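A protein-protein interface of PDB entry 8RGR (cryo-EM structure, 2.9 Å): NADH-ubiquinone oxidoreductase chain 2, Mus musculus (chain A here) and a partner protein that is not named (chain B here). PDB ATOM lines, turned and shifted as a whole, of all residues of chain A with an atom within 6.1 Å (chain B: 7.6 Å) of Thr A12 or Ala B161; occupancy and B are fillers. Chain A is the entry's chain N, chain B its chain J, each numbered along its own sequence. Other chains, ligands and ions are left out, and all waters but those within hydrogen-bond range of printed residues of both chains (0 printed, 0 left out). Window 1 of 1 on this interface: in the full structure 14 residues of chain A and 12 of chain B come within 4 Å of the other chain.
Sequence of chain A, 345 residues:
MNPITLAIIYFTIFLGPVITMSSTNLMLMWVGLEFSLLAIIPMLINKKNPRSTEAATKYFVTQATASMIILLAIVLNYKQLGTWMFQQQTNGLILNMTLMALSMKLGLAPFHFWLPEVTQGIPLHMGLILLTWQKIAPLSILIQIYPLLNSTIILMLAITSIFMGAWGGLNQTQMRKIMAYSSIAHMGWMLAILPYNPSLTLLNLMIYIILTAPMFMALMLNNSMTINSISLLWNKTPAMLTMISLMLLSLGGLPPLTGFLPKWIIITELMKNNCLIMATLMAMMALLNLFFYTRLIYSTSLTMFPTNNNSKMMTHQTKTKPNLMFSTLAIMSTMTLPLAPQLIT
Among the printed residues, merely in contact across the chains: Ile A8 with Trp B157 (3.6 Å), Ile A8 with Phe B164 (3.9 Å), Phe A11 with Trp B157 (3.5 Å), Thr A12 with Ala B161 (3.8 Å), Phe A35 with Trp B157 (3.9 Å), Phe A35 with Ser B158 (3.5 Å) and Ala A39 with Ile B165 (3.8 Å).
Thr A12 touches just these residues of chain B: Trp B157 and Ala B161.
Ala B161 touches just one residue of chain A: Thr A12.
Printed residues of chain B within 4 Å of Ile A8: Trp B157 (3.6 Å) and Phe B164 (3.9 Å).
Of the printed residues of chain B, Phe A11 touches Trp B157.
Of the printed residues of chain B, Ala A39 touches Ile B165 (3.8 Å).
Gly A16 touches none of the printed residues of chain B.
The nearest printed residue of chain B that does not touch Phe A35 is Ala B155 (5.3 Å).
The indole nitrogen of Trp B157 is in hydrogen-bond range of the side-chain hydroxyl of Thr A12, 3.0 Å away.
The backbone carbonyl oxygen (O) of Ile A8 is in hydrogen-bond range of the side-chain hydroxyl (OG1) of Thr A12 (2.7 Å).
Of the 14 printed residues of chain A, 5 touch a printed residue of chain B.
Hydrophobic or aromatic side chains of chain A that line the printed part of chain B: Ile A8, Phe A11 and Phe A35.
Along chain B the printed residues that touch a printed residue of chain A span positions 157 to 165.
Among the printed residues, 8 pairs touch across the chains.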
ATOM      1  N   ALA A   7      18.798  -0.269  12.108  1.00  0.00           N
ATOM      2  CA  ALA A   7      19.576  -0.353  13.334  1.00  0.00           C
ATOM      3  C   ALA A   7      18.710  -0.780  14.506  1.00  0.00           C
ATOM      4  O   ALA A   7      19.122  -1.630  15.300  1.00  0.00           O
ATOM      5  CB  ALA A   7      20.247   0.988  13.623  1.00  0.00           C
ATOM      6  N   ILE A   8      17.497  -0.228  14.613  1.00  0.00           N
ATOM      7  CA  ILE A   8      16.616  -0.578  15.728  1.00  0.00           C
ATOM      8  C   ILE A   8      16.235  -2.055  15.675  1.00  0.00           C
ATOM      9  O   ILE A   8      16.354  -2.782  16.671  1.00  0.00           O
ATOM     10  CB  ILE A   8      15.369   0.323  15.737  1.00  0.00           C
ATOM     11  CG1 ILE A   8      15.751   1.773  16.025  1.00  0.00           C
ATOM     12  CG2 ILE A   8      14.374  -0.161  16.769  1.00  0.00           C
ATOM     13  CD1 ILE A   8      16.430   1.974  17.343  1.00  0.00           C
ATOM     14  N   ILE A   9      15.819  -2.528  14.497  1.00  0.00           N
ATOM     15  CA  ILE A   9      15.350  -3.903  14.368  1.00  0.00           C
ATOM     16  C   ILE A   9      16.497  -4.890  14.552  1.00  0.00           C
ATOM     17  O   ILE A   9      16.361  -5.882  15.280  1.00  0.00           O
ATOM     18  CB  ILE A   9      14.640  -4.092  13.016  1.00  0.00           C
ATOM     19  CG1 ILE A   9      13.287  -3.378  13.028  1.00  0.00           C
ATOM     20  CG2 ILE A   9      14.447  -5.558  12.705  1.00  0.00           C
ATOM     21  CD1 ILE A   9      12.510  -3.521  11.742  1.00  0.00           C
ATOM     22  N   TYR A  10      17.648  -4.632  13.923  1.00  0.00           N
ATOM     23  CA  TYR A  10      18.772  -5.548  14.064  1.00  0.00           C
ATOM     24  C   TYR A  10      19.347  -5.530  15.472  1.00  0.00           C
ATOM     25  O   TYR A  10      19.758  -6.580  15.980  1.00  0.00           O
ATOM     26  CB  TYR A  10      19.849  -5.219  13.038  1.00  0.00           C
ATOM     27  CG  TYR A  10      19.608  -5.877  11.705  1.00  0.00           C
ATOM     28  CD1 TYR A  10      19.167  -7.189  11.634  1.00  0.00           C
ATOM     29  CD2 TYR A  10      19.807  -5.186  10.520  1.00  0.00           C
ATOM     30  CE1 TYR A  10      18.940  -7.800  10.421  1.00  0.00           C
ATOM     31  CE2 TYR A  10      19.581  -5.788   9.301  1.00  0.00           C
ATOM     32  CZ  TYR A  10      19.148  -7.096   9.258  1.00  0.00           C
ATOM     33  OH  TYR A  10      18.921  -7.703   8.046  1.00  0.00           O
ATOM     34  N   PHE A  11      19.360  -4.369  16.132  1.00  0.00           N
ATOM     35  CA  PHE A  11      19.833  -4.323  17.506  1.00  0.00           C
ATOM     36  C   PHE A  11      18.899  -5.075  18.436  1.00  0.00           C
ATOM     37  O   PHE A  11      19.356  -5.734  19.371  1.00  0.00           O
ATOM     38  CB  PHE A  11      19.991  -2.880  17.974  1.00  0.00           C
ATOM     39  CG  PHE A  11      20.392  -2.761  19.410  1.00  0.00           C
ATOM     40  CD1 PHE A  11      21.673  -3.092  19.810  1.00  0.00           C
ATOM     41  CD2 PHE A  11      19.491  -2.327  20.361  1.00  0.00           C
ATOM     42  CE1 PHE A  11      22.046  -2.990  21.133  1.00  0.00           C
ATOM     43  CE2 PHE A  11      19.858  -2.222  21.685  1.00  0.00           C
ATOM     44  CZ  PHE A  11      21.138  -2.553  22.071  1.00  0.00           C
ATOM     45  N   THR A  12      17.588  -5.004  18.201  1.00  0.00           N
ATOM     46  CA  THR A  12      16.671  -5.748  19.057  1.00  0.00           C
ATOM     47  C   THR A  12      16.750  -7.249  18.783  1.00  0.00           C
ATOM     48  O   THR A  12      16.641  -8.062  19.714  1.00  0.00           O
ATOM     49  CB  THR A  12      15.252  -5.222  18.876  1.00  0.00           C
ATOM     50  OG1 THR A  12      15.278  -3.791  18.890  1.00  0.00           O
ATOM     51  CG2 THR A  12      14.365  -5.701  20.005  1.00  0.00           C
ATOM     52  N   ILE A  13      16.965  -7.629  17.519  1.00  0.00           N
ATOM     53  CA  ILE A  13      17.198  -9.031  17.165  1.00  0.00           C
ATOM     54  C   ILE A  13      18.430  -9.560  17.882  1.00  0.00           C
ATOM     55  O   ILE A  13      18.422 -10.668  18.430  1.00  0.00           O
ATOM     56  CB  ILE A  13      17.327  -9.181  15.635  1.00  0.00           C
ATOM     57  CG1 ILE A  13      15.952  -9.244  14.973  1.00  0.00           C
ATOM     58  CG2 ILE A  13      18.130 -10.418  15.256  1.00  0.00           C
ATOM     59  CD1 ILE A  13      16.001  -9.430  13.473  1.00  0.00           C
ATOM     60  N   PHE A  14      19.507  -8.775  17.895  1.00  0.00           N
ATOM     61  CA  PHE A  14      20.700  -9.155  18.640  1.00  0.00           C
ATOM     62  C   PHE A  14      20.437  -9.184  20.142  1.00  0.00           C
ATOM     63  O   PHE A  14      20.908 -10.085  20.842  1.00  0.00           O
ATOM     64  CB  PHE A  14      21.838  -8.193  18.306  1.00  0.00           C
ATOM     65  CG  PHE A  14      23.061  -8.388  19.141  1.00  0.00           C
ATOM     66  CD1 PHE A  14      23.890  -9.474  18.931  1.00  0.00           C
ATOM     67  CD2 PHE A  14      23.391  -7.477  20.129  1.00  0.00           C
ATOM     68  CE1 PHE A  14      25.019  -9.655  19.697  1.00  0.00           C
ATOM     69  CE2 PHE A  14      24.518  -7.654  20.898  1.00  0.00           C
ATOM     70  CZ  PHE A  14      25.333  -8.743  20.680  1.00  0.00           C
ATOM     71  N   LEU A  15      19.671  -8.217  20.646  1.00  0.00           N
ATOM     72  CA  LEU A  15      19.532  -8.019  22.082  1.00  0.00           C
ATOM     73  C   LEU A  15      18.658  -9.081  22.730  1.00  0.00           C
ATOM     74  O   LEU A  15      18.813  -9.351  23.927  1.00  0.00           O
ATOM     75  CB  LEU A  15      18.955  -6.630  22.347  1.00  0.00           C
ATOM     76  CG  LEU A  15      18.931  -6.112  23.782  1.00  0.00           C
ATOM     77  CD1 LEU A  15      20.332  -5.757  24.239  1.00  0.00           C
ATOM     78  CD2 LEU A  15      17.999  -4.922  23.901  1.00  0.00           C
ATOM     79  N   GLY A  16      17.734  -9.673  21.976  1.00  0.00           N
ATOM     80  CA  GLY A  16      16.845 -10.685  22.507  1.00  0.00           C
ATOM     81  C   GLY A  16      17.549 -11.880  23.128  1.00  0.00           C
ATOM     82  O   GLY A  16      17.462 -12.121  24.341  1.00  0.00           O
ATOM     83  N   PRO A  17      18.250 -12.661  22.302  1.00  0.00           N
ATOM     84  CA  PRO A  17      19.041 -13.778  22.840  1.00  0.00           C
ATOM     85  C   PRO A  17      20.125 -13.365  23.817  1.00  0.00           C
ATOM     86  O   PRO A  17      20.441 -14.147  24.718  1.00  0.00           O
ATOM     87  CB  PRO A  17      19.634 -14.412  21.579  1.00  0.00           C
ATOM     88  CG  PRO A  17      18.634 -14.126  20.535  1.00  0.00           C
ATOM     89  CD  PRO A  17      18.103 -12.759  20.842  1.00  0.00           C
ATOM     90  N   PHE A  35      11.495 -10.182  22.805  1.00  0.00           N
ATOM     91  CA  PHE A  35      12.297  -9.281  21.989  1.00  0.00           C
ATOM     92  C   PHE A  35      12.692  -9.933  20.679  1.00  0.00           C
ATOM     93  O   PHE A  35      12.543  -9.328  19.611  1.00  0.00           O
ATOM     94  CB  PHE A  35      13.548  -8.862  22.754  1.00  0.00           C
ATOM     95  CG  PHE A  35      13.366  -7.644  23.589  1.00  0.00           C
ATOM     96  CD1 PHE A  35      12.512  -6.640  23.189  1.00  0.00           C
ATOM     97  CD2 PHE A  35      14.055  -7.500  24.775  1.00  0.00           C
ATOM     98  CE1 PHE A  35      12.350  -5.517  23.962  1.00  0.00           C
ATOM     99  CE2 PHE A  35      13.895  -6.379  25.549  1.00  0.00           C
ATOM    100  CZ  PHE A  35      13.041  -5.386  25.143  1.00  0.00           C
ATOM    101  N   SER A  36      13.170 -11.179  20.746  1.00  0.00           N
ATOM    102  CA  SER A  36      13.611 -11.881  19.544  1.00  0.00           C
ATOM    103  C   SER A  36      12.463 -12.067  18.559  1.00  0.00           C
ATOM    104  O   SER A  36      12.597 -11.758  17.367  1.00  0.00           O
ATOM    105  CB  SER A  36      14.220 -13.227  19.926  1.00  0.00           C
ATOM    106  OG  SER A  36      14.860 -13.826  18.817  1.00  0.00           O
ATOM    107  N   ALA A  39      11.094  -8.563  17.194  1.00  0.00           N
ATOM    108  CA  ALA A  39      12.053  -7.913  16.319  1.00  0.00           C
ATOM    109  C   ALA A  39      12.244  -8.672  15.017  1.00  0.00           C
ATOM    110  O   ALA A  39      12.536  -8.055  13.988  1.00  0.00           O
ATOM    111  CB  ALA A  39      13.382  -7.761  17.045  1.00  0.00           C
ATOM    112  N   ALA B 155      11.193  -2.626  29.305  1.00  0.00           N
ATOM    113  CA  ALA B 155       9.822  -2.282  28.936  1.00  0.00           C
ATOM    114  C   ALA B 155       9.782  -1.093  27.976  1.00  0.00           C
ATOM    115  O   ALA B 155       9.060  -1.114  26.964  1.00  0.00           O
ATOM    116  CB  ALA B 155       9.006  -1.993  30.193  1.00  0.00           C
ATOM    117  N   GLY B 156      10.569  -0.055  28.268  1.00  0.00           N
ATOM    118  CA  GLY B 156      10.603   1.107  27.396  1.00  0.00           C
ATOM    119  C   GLY B 156      11.153   0.796  26.018  1.00  0.00           C
ATOM    120  O   GLY B 156      10.628   1.277  25.007  1.00  0.00           O
ATOM    121  N   TRP B 157      12.204  -0.025  25.952  1.00  0.00           N
ATOM    122  CA  TRP B 157      12.734  -0.416  24.656  1.00  0.00           C
ATOM    123  C   TRP B 157      11.765  -1.311  23.908  1.00  0.00           C
ATOM    124  O   TRP B 157      11.719  -1.262  22.677  1.00  0.00           O
ATOM    125  CB  TRP B 157      14.079  -1.121  24.804  1.00  0.00           C
ATOM    126  CG  TRP B 157      14.698  -1.384  23.481  1.00  0.00           C
ATOM    127  CD1 TRP B 157      14.647  -2.541  22.767  1.00  0.00           C
ATOM    128  CD2 TRP B 157      15.432  -0.453  22.685  1.00  0.00           C
ATOM    129  NE1 TRP B 157      15.318  -2.393  21.580  1.00  0.00           N
ATOM    130  CE2 TRP B 157      15.811  -1.118  21.508  1.00  0.00           C
ATOM    131  CE3 TRP B 157      15.812   0.878  22.860  1.00  0.00           C
ATOM    132  CZ2 TRP B 157      16.549  -0.499  20.511  1.00  0.00           C
ATOM    133  CZ3 TRP B 157      16.547   1.490  21.870  1.00  0.00           C
ATOM    134  CH2 TRP B 157      16.909   0.803  20.712  1.00  0.00           C
ATOM    135  N   SER B 158      10.985  -2.126  24.624  1.00  0.00           N
ATOM    136  CA  SER B 158       9.952  -2.917  23.966  1.00  0.00           C
ATOM    137  C   SER B 158       8.930  -2.023  23.292  1.00  0.00           C
ATOM    138  O   SER B 158       8.568  -2.253  22.137  1.00  0.00           O
ATOM    139  CB  SER B 158       9.265  -3.833  24.971  1.00  0.00           C
ATOM    140  OG  SER B 158       8.496  -3.075  25.885  1.00  0.00           O
ATOM    141  N   LEU B 159       8.492  -0.968  23.979  1.00  0.00           N
ATOM    142  CA  LEU B 159       7.516  -0.062  23.374  1.00  0.00           C
ATOM    143  C   LEU B 159       8.112   0.720  22.201  1.00  0.00           C
ATOM    144  O   LEU B 159       7.459   0.890  21.162  1.00  0.00           O
ATOM    145  CB  LEU B 159       6.962   0.872  24.441  1.00  0.00           C
ATOM    146  CG  LEU B 159       6.221   0.056  25.500  1.00  0.00           C
ATOM    147  CD1 LEU B 159       5.936   0.866  26.741  1.00  0.00           C
ATOM    148  CD2 LEU B 159       4.939  -0.501  24.920  1.00  0.00           C
ATOM    149  N   PHE B 160       9.359   1.174  22.339  1.00  0.00           N
ATOM    150  CA  PHE B 160      10.017   1.938  21.279  1.00  0.00           C
ATOM    151  C   PHE B 160      10.243   1.088  20.029  1.00  0.00           C
ATOM    152  O   PHE B 160       9.860   1.470  18.904  1.00  0.00           O
ATOM    153  CB  PHE B 160      11.340   2.467  21.828  1.00  0.00           C
ATOM    154  CG  PHE B 160      12.011   3.475  20.959  1.00  0.00           C
ATOM    155  CD1 PHE B 160      11.384   4.663  20.643  1.00  0.00           C
ATOM    156  CD2 PHE B 160      13.294   3.252  20.495  1.00  0.00           C
ATOM    157  CE1 PHE B 160      12.014   5.600  19.855  1.00  0.00           C
ATOM    158  CE2 PHE B 160      13.929   4.184  19.708  1.00  0.00           C
ATOM    159  CZ  PHE B 160      13.290   5.361  19.390  1.00  0.00           C
ATOM    160  N   ALA B 161      10.852  -0.086  20.215  1.00  0.00           N
ATOM    161  CA  ALA B 161      11.040  -1.019  19.120  1.00  0.00           C
ATOM    162  C   ALA B 161       9.711  -1.481  18.554  1.00  0.00           C
ATOM    163  O   ALA B 161       9.619  -1.734  17.356  1.00  0.00           O
ATOM    164  CB  ALA B 161      11.865  -2.217  19.584  1.00  0.00           C
ATOM    165  N   GLY B 162       8.669  -1.564  19.384  1.00  0.00           N
ATOM    166  CA  GLY B 162       7.359  -1.919  18.875  1.00  0.00           C
ATOM    167  C   GLY B 162       6.787  -0.865  17.952  1.00  0.00           C
ATOM    168  O   GLY B 162       6.128  -1.197  16.966  1.00  0.00           O
ATOM    169  N   ILE B 163       7.026   0.413  18.259  1.00  0.00           N
ATOM    170  CA  ILE B 163       6.620   1.486  17.348  1.00  0.00           C
ATOM    171  C   ILE B 163       7.317   1.330  16.002  1.00  0.00           C
ATOM    172  O   ILE B 163       6.680   1.377  14.935  1.00  0.00           O
ATOM    173  CB  ILE B 163       6.918   2.863  17.968  1.00  0.00           C
ATOM    174  CG1 ILE B 163       6.006   3.127  19.163  1.00  0.00           C
ATOM    175  CG2 ILE B 163       6.754   3.959  16.935  1.00  0.00           C
ATOM    176  CD1 ILE B 163       6.238   4.463  19.819  1.00  0.00           C
ATOM    177  N   PHE B 164       8.633   1.103  16.036  1.00  0.00           N
ATOM    178  CA  PHE B 164       9.367   0.906  14.784  1.00  0.00           C
ATOM    179  C   PHE B 164       8.882  -0.336  14.036  1.00  0.00           C
ATOM    180  O   PHE B 164       8.740  -0.321  12.805  1.00  0.00           O
ATOM    181  CB  PHE B 164      10.864   0.813  15.063  1.00  0.00           C
ATOM    182  CG  PHE B 164      11.529   2.144  15.202  1.00  0.00           C
ATOM    183  CD1 PHE B 164      11.377   2.889  16.354  1.00  0.00           C
ATOM    184  CD2 PHE B 164      12.303   2.654  14.178  1.00  0.00           C
ATOM    185  CE1 PHE B 164      11.984   4.113  16.479  1.00  0.00           C
ATOM    186  CE2 PHE B 164      12.917   3.879  14.303  1.00  0.00           C
ATOM    187  CZ  PHE B 164      12.755   4.608  15.456  1.00  0.00           C
ATOM    188  N   ILE B 165       8.576  -1.397  14.780  1.00  0.00           N
ATOM    189  CA  ILE B 165       8.154  -2.665  14.201  1.00  0.00           C
ATOM    190  C   ILE B 165       6.802  -2.523  13.514  1.00  0.00           C
ATOM    191  O   ILE B 165       6.617  -2.999  12.390  1.00  0.00           O
ATOM    192  CB  ILE B 165       8.136  -3.747  15.299  1.00  0.00           C
ATOM    193  CG1 ILE B 165       9.534  -4.334  15.494  1.00  0.00           C
ATOM    194  CG2 ILE B 165       7.112  -4.835  15.011  1.00  0.00           C
ATOM    195  CD1 ILE B 165       9.760  -4.917  16.867  1.00  0.00           C
ATOM    196  N   ILE B 166       5.841  -1.866  14.169  1.00  0.00           N
ATOM    197  CA  ILE B 166       4.516  -1.745  13.570  1.00  0.00           C
ATOM    198  C   ILE B 166       4.551  -0.817  12.366  1.00  0.00           C
ATOM    199  O   ILE B 166       3.839  -1.057  11.379  1.00  0.00           O
ATOM    200  CB  ILE B 166       3.464  -1.302  14.605  1.00  0.00           C
ATOM    201  CG1 ILE B 166       3.812   0.059  15.205  1.00  0.00           C
ATOM    202  CG2 ILE B 166       3.339  -2.353  15.690  1.00  0.00           C
ATOM    203  CD1 ILE B 166       2.649   0.902  15.614  1.00  0.00           C
ATOM    204  N   ILE B 167       5.391   0.227  12.401  1.00  0.00           N
ATOM    205  CA  ILE B 167       5.541   1.084  11.226  1.00  0.00           C
ATOM    206  C   ILE B 167       6.102   0.283  10.057  1.00  0.00           C
ATOM    207  O   ILE B 167       5.614   0.381   8.925  1.00  0.00           O
ATOM    208  CB  ILE B 167       6.415   2.306  11.557  1.00  0.00           C
ATOM    209  CG1 ILE B 167       5.652   3.265  12.467  1.00  0.00           C
ATOM    210  CG2 ILE B 167       6.835   3.029  10.295  1.00  0.00           C
ATOM    211  CD1 ILE B 167       6.424   4.508  12.827  1.00  0.00           C
ATOM    212  N   GLU B 168       7.099  -0.564  10.322  1.00  0.00           N
ATOM    213  CA  GLU B 168       7.679  -1.341   9.234  1.00  0.00           C
ATOM    214  C   GLU B 168       6.758  -2.445   8.729  1.00  0.00           C
ATOM    215  O   GLU B 168       6.806  -2.779   7.541  1.00  0.00           O
ATOM    216  CB  GLU B 168       9.013  -1.940   9.663  1.00  0.00           C
ATOM    217  CG  GLU B 168      10.115  -0.921   9.706  1.00  0.00           C
ATOM    218  CD  GLU B 168      10.255  -0.171   8.397  1.00  0.00           C
ATOM    219  OE1 GLU B 168      10.285  -0.824   7.332  1.00  0.00           O
ATOM    220  OE2 GLU B 168      10.335   1.076   8.433  1.00  0.00           O
